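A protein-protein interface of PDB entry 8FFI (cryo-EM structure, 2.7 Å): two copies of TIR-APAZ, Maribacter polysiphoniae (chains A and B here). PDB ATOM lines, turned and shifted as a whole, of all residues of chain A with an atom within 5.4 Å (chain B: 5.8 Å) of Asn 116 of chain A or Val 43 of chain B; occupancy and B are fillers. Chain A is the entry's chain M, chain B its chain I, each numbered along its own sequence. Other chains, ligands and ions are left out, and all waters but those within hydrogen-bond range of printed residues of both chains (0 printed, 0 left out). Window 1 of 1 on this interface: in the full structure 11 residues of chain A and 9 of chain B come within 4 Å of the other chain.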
ATOM      1  N   ASP A  91     -17.614  -6.488  28.520  1.00  0.00           N
ATOM      2  CA  ASP A  91     -16.749  -6.732  27.373  1.00  0.00           C
ATOM      3  C   ASP A  91     -15.454  -7.432  27.768  1.00  0.00           C
ATOM      4  O   ASP A  91     -14.900  -8.195  26.969  1.00  0.00           O
ATOM      5  CB  ASP A  91     -16.440  -5.414  26.662  1.00  0.00           C
ATOM      6  CG  ASP A  91     -16.050  -5.612  25.210  1.00  0.00           C
ATOM      7  OD1 ASP A  91     -15.964  -6.777  24.766  1.00  0.00           O
ATOM      8  OD2 ASP A  91     -15.832  -4.601  24.509  1.00  0.00           O
ATOM      9  N   LYS A  92     -14.964  -7.198  28.980  1.00  0.00           N
ATOM     10  CA  LYS A  92     -13.691  -7.746  29.448  1.00  0.00           C
ATOM     11  C   LYS A  92     -13.977  -8.709  30.597  1.00  0.00           C
ATOM     12  O   LYS A  92     -13.956  -8.327  31.769  1.00  0.00           O
ATOM     13  CB  LYS A  92     -12.754  -6.621  29.877  1.00  0.00           C
ATOM     14  CG  LYS A  92     -12.790  -5.413  28.955  1.00  0.00           C
ATOM     15  CD  LYS A  92     -11.892  -4.301  29.461  1.00  0.00           C
ATOM     16  CE  LYS A  92     -12.592  -3.463  30.518  1.00  0.00           C
ATOM     17  NZ  LYS A  92     -13.839  -2.837  29.998  1.00  0.00           N
ATOM     18  N   ILE A  95      -9.699 -13.148  30.422  1.00  0.00           N
ATOM     19  CA  ILE A  95      -8.376 -12.551  30.255  1.00  0.00           C
ATOM     20  C   ILE A  95      -7.338 -13.659  30.107  1.00  0.00           C
ATOM     21  O   ILE A  95      -6.882 -14.219  31.115  1.00  0.00           O
ATOM     22  CB  ILE A  95      -8.030 -11.623  31.431  1.00  0.00           C
ATOM     23  CG1 ILE A  95      -9.105 -10.547  31.593  1.00  0.00           C
ATOM     24  CG2 ILE A  95      -6.666 -10.987  31.221  1.00  0.00           C
ATOM     25  CD1 ILE A  95      -8.711  -9.424  32.524  1.00  0.00           C
ATOM     26  N   PRO A  96      -6.944 -14.013  28.885  1.00  0.00           N
ATOM     27  CA  PRO A  96      -5.945 -15.073  28.712  1.00  0.00           C
ATOM     28  C   PRO A  96      -4.574 -14.652  29.223  1.00  0.00           C
ATOM     29  O   PRO A  96      -4.197 -13.478  29.173  1.00  0.00           O
ATOM     30  CB  PRO A  96      -5.924 -15.303  27.195  1.00  0.00           C
ATOM     31  CG  PRO A  96      -7.160 -14.641  26.670  1.00  0.00           C
ATOM     32  CD  PRO A  96      -7.450 -13.510  27.599  1.00  0.00           C
ATOM     33  N   ARG A 114      -9.416 -12.917  19.173  1.00  0.00           N
ATOM     34  CA  ARG A 114      -9.567 -11.480  19.003  1.00  0.00           C
ATOM     35  C   ARG A 114      -9.314 -10.720  20.298  1.00  0.00           C
ATOM     36  O   ARG A 114      -9.534  -9.506  20.346  1.00  0.00           O
ATOM     37  CB  ARG A 114     -10.966 -11.159  18.472  1.00  0.00           C
ATOM     38  CG  ARG A 114     -11.299 -11.830  17.152  1.00  0.00           C
ATOM     39  CD  ARG A 114     -12.693 -11.460  16.676  1.00  0.00           C
ATOM     40  NE  ARG A 114     -12.879 -10.017  16.583  1.00  0.00           N
ATOM     41  CZ  ARG A 114     -12.549  -9.286  15.527  1.00  0.00           C
ATOM     42  NH1 ARG A 114     -12.007  -9.831  14.450  1.00  0.00           N
ATOM     43  NH2 ARG A 114     -12.771  -7.975  15.551  1.00  0.00           N
ATOM     44  N   LEU A 115      -8.855 -11.401  21.341  1.00  0.00           N
ATOM     45  CA  LEU A 115      -8.729 -10.818  22.667  1.00  0.00           C
ATOM     46  C   LEU A 115      -7.281 -10.447  22.960  1.00  0.00           C
ATOM     47  O   LEU A 115      -6.345 -11.109  22.506  1.00  0.00           O
ATOM     48  CB  LEU A 115      -9.245 -11.788  23.734  1.00  0.00           C
ATOM     49  CG  LEU A 115     -10.707 -11.648  24.169  1.00  0.00           C
ATOM     50  CD1 LEU A 115     -11.652 -11.682  22.978  1.00  0.00           C
ATOM     51  CD2 LEU A 115     -11.073 -12.731  25.172  1.00  0.00           C
ATOM     52  N   ASN A 116      -7.108  -9.374  23.730  1.00  0.00           N
ATOM     53  CA  ASN A 116      -5.784  -8.880  24.099  1.00  0.00           C
ATOM     54  C   ASN A 116      -5.267  -9.686  25.285  1.00  0.00           C
ATOM     55  O   ASN A 116      -5.809  -9.597  26.391  1.00  0.00           O
ATOM     56  CB  ASN A 116      -5.851  -7.391  24.426  1.00  0.00           C
ATOM     57  CG  ASN A 116      -4.483  -6.761  24.559  1.00  0.00           C
ATOM     58  OD1 ASN A 116      -3.504  -7.253  23.999  1.00  0.00           O
ATOM     59  ND2 ASN A 116      -4.407  -5.664  25.301  1.00  0.00           N
ATOM     60  N   ALA A 117      -4.214 -10.464  25.061  1.00  0.00           N
ATOM     61  CA  ALA A 117      -3.693 -11.387  26.059  1.00  0.00           C
ATOM     62  C   ALA A 117      -2.517 -10.779  26.814  1.00  0.00           C
ATOM     63  O   ALA A 117      -1.742  -9.989  26.268  1.00  0.00           O
ATOM     64  CB  ALA A 117      -3.263 -12.702  25.407  1.00  0.00           C
ATOM     65  N   ILE A 118      -2.395 -11.160  28.083  1.00  0.00           N
ATOM     66  CA  ILE A 118      -1.279 -10.738  28.919  1.00  0.00           C
ATOM     67  C   ILE A 118      -0.109 -11.691  28.711  1.00  0.00           C
ATOM     68  O   ILE A 118      -0.275 -12.917  28.726  1.00  0.00           O
ATOM     69  CB  ILE A 118      -1.704 -10.680  30.397  1.00  0.00           C
ATOM     70  CG1 ILE A 118      -2.633  -9.489  30.637  1.00  0.00           C
ATOM     71  CG2 ILE A 118      -0.490 -10.596  31.304  1.00  0.00           C
ATOM     72  CD1 ILE A 118      -3.365  -9.538  31.958  1.00  0.00           C
ATOM     73  N   LEU B  39      -5.026   0.722  25.768  1.00  0.00           N
ATOM     74  CA  LEU B  39      -5.727  -0.493  25.382  1.00  0.00           C
ATOM     75  C   LEU B  39      -5.904  -1.398  26.594  1.00  0.00           C
ATOM     76  O   LEU B  39      -5.003  -1.534  27.426  1.00  0.00           O
ATOM     77  CB  LEU B  39      -4.964  -1.222  24.277  1.00  0.00           C
ATOM     78  CG  LEU B  39      -5.688  -2.380  23.589  1.00  0.00           C
ATOM     79  CD1 LEU B  39      -7.050  -1.940  23.083  1.00  0.00           C
ATOM     80  CD2 LEU B  39      -4.845  -2.929  22.450  1.00  0.00           C
ATOM     81  N   ASP B  40      -7.076  -2.016  26.696  1.00  0.00           N
ATOM     82  CA  ASP B  40      -7.404  -2.848  27.841  1.00  0.00           C
ATOM     83  C   ASP B  40      -6.893  -4.273  27.645  1.00  0.00           C
ATOM     84  O   ASP B  40      -6.501  -4.681  26.549  1.00  0.00           O
ATOM     85  CB  ASP B  40      -8.911  -2.853  28.083  1.00  0.00           C
ATOM     86  CG  ASP B  40      -9.361  -1.712  28.973  1.00  0.00           C
ATOM     87  OD1 ASP B  40      -8.969  -1.693  30.158  1.00  0.00           O
ATOM     88  OD2 ASP B  40     -10.110  -0.840  28.488  1.00  0.00           O
ATOM     89  N   LYS B  41      -6.903  -5.033  28.734  1.00  0.00           N
ATOM     90  CA  LYS B  41      -6.446  -6.415  28.739  1.00  0.00           C
ATOM     91  C   LYS B  41      -7.657  -7.337  28.662  1.00  0.00           C
ATOM     92  O   LYS B  41      -8.568  -7.242  29.491  1.00  0.00           O
ATOM     93  CB  LYS B  41      -5.622  -6.709  29.992  1.00  0.00           C
ATOM     94  CG  LYS B  41      -4.458  -5.754  30.199  1.00  0.00           C
ATOM     95  CD  LYS B  41      -3.301  -6.087  29.275  1.00  0.00           C
ATOM     96  CE  LYS B  41      -2.294  -4.953  29.223  1.00  0.00           C
ATOM     97  NZ  LYS B  41      -0.921  -5.447  28.933  1.00  0.00           N
ATOM     98  N   GLY B  42      -7.665  -8.221  27.668  1.00  0.00           N
ATOM     99  CA  GLY B  42      -8.783  -9.122  27.479  1.00  0.00           C
ATOM    100  C   GLY B  42      -9.955  -8.539  26.727  1.00  0.00           C
ATOM    101  O   GLY B  42     -11.073  -9.045  26.862  1.00  0.00           O
ATOM    102  N   VAL B  43      -9.739  -7.491  25.940  1.00  0.00           N
ATOM    103  CA  VAL B  43     -10.798  -6.840  25.181  1.00  0.00           C
ATOM    104  C   VAL B  43     -10.562  -7.097  23.699  1.00  0.00           C
ATOM    105  O   VAL B  43      -9.425  -7.285  23.253  1.00  0.00           O
ATOM    106  CB  VAL B  43     -10.852  -5.325  25.484  1.00  0.00           C
ATOM    107  CG1 VAL B  43      -9.615  -4.622  24.942  1.00  0.00           C
ATOM    108  CG2 VAL B  43     -12.125  -4.698  24.935  1.00  0.00           C
ATOM    109  N   ASP B  44     -11.652  -7.125  22.933  1.00  0.00           N
ATOM    110  CA  ASP B  44     -11.557  -7.209  21.481  1.00  0.00           C
ATOM    111  C   ASP B  44     -10.914  -5.928  20.965  1.00  0.00           C
ATOM    112  O   ASP B  44     -11.543  -4.865  20.967  1.00  0.00           O
ATOM    113  CB  ASP B  44     -12.939  -7.421  20.873  1.00  0.00           C
ATOM    114  CG  ASP B  44     -12.882  -7.835  19.417  1.00  0.00           C
ATOM    115  OD1 ASP B  44     -11.772  -7.862  18.843  1.00  0.00           O
ATOM    116  OD2 ASP B  44     -13.949  -8.137  18.845  1.00  0.00           O
ATOM    117  N   PHE B  45      -9.661  -6.022  20.520  1.00  0.00           N
ATOM    118  CA  PHE B  45      -8.864  -4.821  20.301  1.00  0.00           C
ATOM    119  C   PHE B  45      -9.083  -4.190  18.932  1.00  0.00           C
ATOM    120  O   PHE B  45      -9.063  -2.961  18.821  1.00  0.00           O
ATOM    121  CB  PHE B  45      -7.375  -5.122  20.511  1.00  0.00           C
ATOM    122  CG  PHE B  45      -6.873  -6.321  19.760  1.00  0.00           C
ATOM    123  CD1 PHE B  45      -6.985  -7.592  20.298  1.00  0.00           C
ATOM    124  CD2 PHE B  45      -6.269  -6.176  18.524  1.00  0.00           C
ATOM    125  CE1 PHE B  45      -6.518  -8.695  19.613  1.00  0.00           C
ATOM    126  CE2 PHE B  45      -5.798  -7.276  17.833  1.00  0.00           C
ATOM    127  CZ  PHE B  45      -5.923  -8.537  18.379  1.00  0.00           C
ATOM    128  N   ASN B  48     -12.388  -2.277  19.216  1.00  0.00           N
ATOM    129  CA  ASN B  48     -12.223  -1.085  20.042  1.00  0.00           C
ATOM    130  C   ASN B  48     -11.422  -0.012  19.314  1.00  0.00           C
ATOM    131  O   ASN B  48     -11.749   1.177  19.397  1.00  0.00           O
ATOM    132  CB  ASN B  48     -11.550  -1.455  21.364  1.00  0.00           C
ATOM    133  CG  ASN B  48     -11.536  -0.305  22.352  1.00  0.00           C
ATOM    134  OD1 ASN B  48     -12.312   0.642  22.231  1.00  0.00           O
ATOM    135  ND2 ASN B  48     -10.651  -0.383  23.339  1.00  0.00           N
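Gly 42 of chain B touches Asp 91 of chain A (O to O, 3.9 Å). OD2 of Asp 91 of chain A touches CG2 of Val 43 of chain B, at 3.7 Å. CD of Lys 92 of chain A touches CB of Asp 40 of chain B, at 3.6 Å. CA of Lys 92 of chain A touches O of Gly 42 of chain B (3.9 Å). CB of Val 43 of chain B touches CG of Lys 92 of chain A, at 3.98 Å. CD1 of Ile 95 of chain A touches O of Lys 41 of chain B (3.7 Å). O of Val 43 of chain B touches O of Arg 114 of chain A (3.7 Å). Leu 115 of chain A touches Gly 42 of chain B. Leu 39 of chain B touches Asn 116 of chain A. Ile 118 of chain A touches Lys 41 of chain B (CG1 to CD, 3.7 Å).
No position is printed for both chains.
O of Pro 96 of chain A is in hydrogen-bond range of N of Ile 118 of chain A (3.1 Å).
The side-chain amide nitrogen (ND2) of Asn 116 of chain A sits at hydrogen-bond distance from the backbone carbonyl oxygen (O) of Asp 40 of chain B, 2.6 Å away. The backbone NH of Gly 42 of chain B lies within hydrogen-bond range of the backbone carbonyl oxygen of Asn 116 of chain A (2.6 Å). The backbone NH (N) of Asn 116 of chain A lies within hydrogen-bond range of the backbone carbonyl oxygen (O) of Val 43 of chain B, at 3.2 Å. NE of Arg 114 of chain A is in salt-bridge range of OD2 of Asp 44 of chain B (3.1 Å). The backbone carbonyl oxygen of Arg 114 of chain A lies close to the backbone NH of Phe 45 of chain B (3.5 Å).
Along chain B the printed residues that touch a printed residue of chain A span positions 39 to 45. Hydrophobic or aromatic side chains of chain A within 4 Å of the printed part of chain B: Ile 95, Leu 115 and Ile 118.
Of chain B, only Leu 39 (3.9 Å), Asp 40 (2.6 Å), Lys 41 (3.7 Å), Gly 42 (2.6 Å), Val 43 (3.2 Å) and Phe 45 (3.9 Å) come within 4 Å of Asn 116 of chain A. Of chain A, only Asp 91 (3.7 Å), Lys 92 (3.98 Å), Arg 114 (3.7 Å), Leu 115 (3.6 Å) and Asn 116 (3.2 Å) come within 4 Å of Val 43 of chain B. Printed residues of chain B within 4 Å of Asp 91 of chain A: Gly 42 and Val 43. Printed residues of chain B within 4 Å of Arg 114 of chain A: Val 43, Asp 44 and Phe 45. Of the printed residues of chain A, Gly 42 of chain B touches Asp 91 (3.9 Å), Lys 92 (3.9 Å), Leu 115 (3.8 Å) and Asn 116 (2.6 Å). Ala 117 of chain A touches none of the printed residues of chain B. The nearest residue of chain B that does not touch Asn 116 of chain A is Asp 44 of chain B (5.1 Å). The nearest printed residue of chain A that does not touch Leu 39 of chain B is Lys 92 of chain A (7.2 Å).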
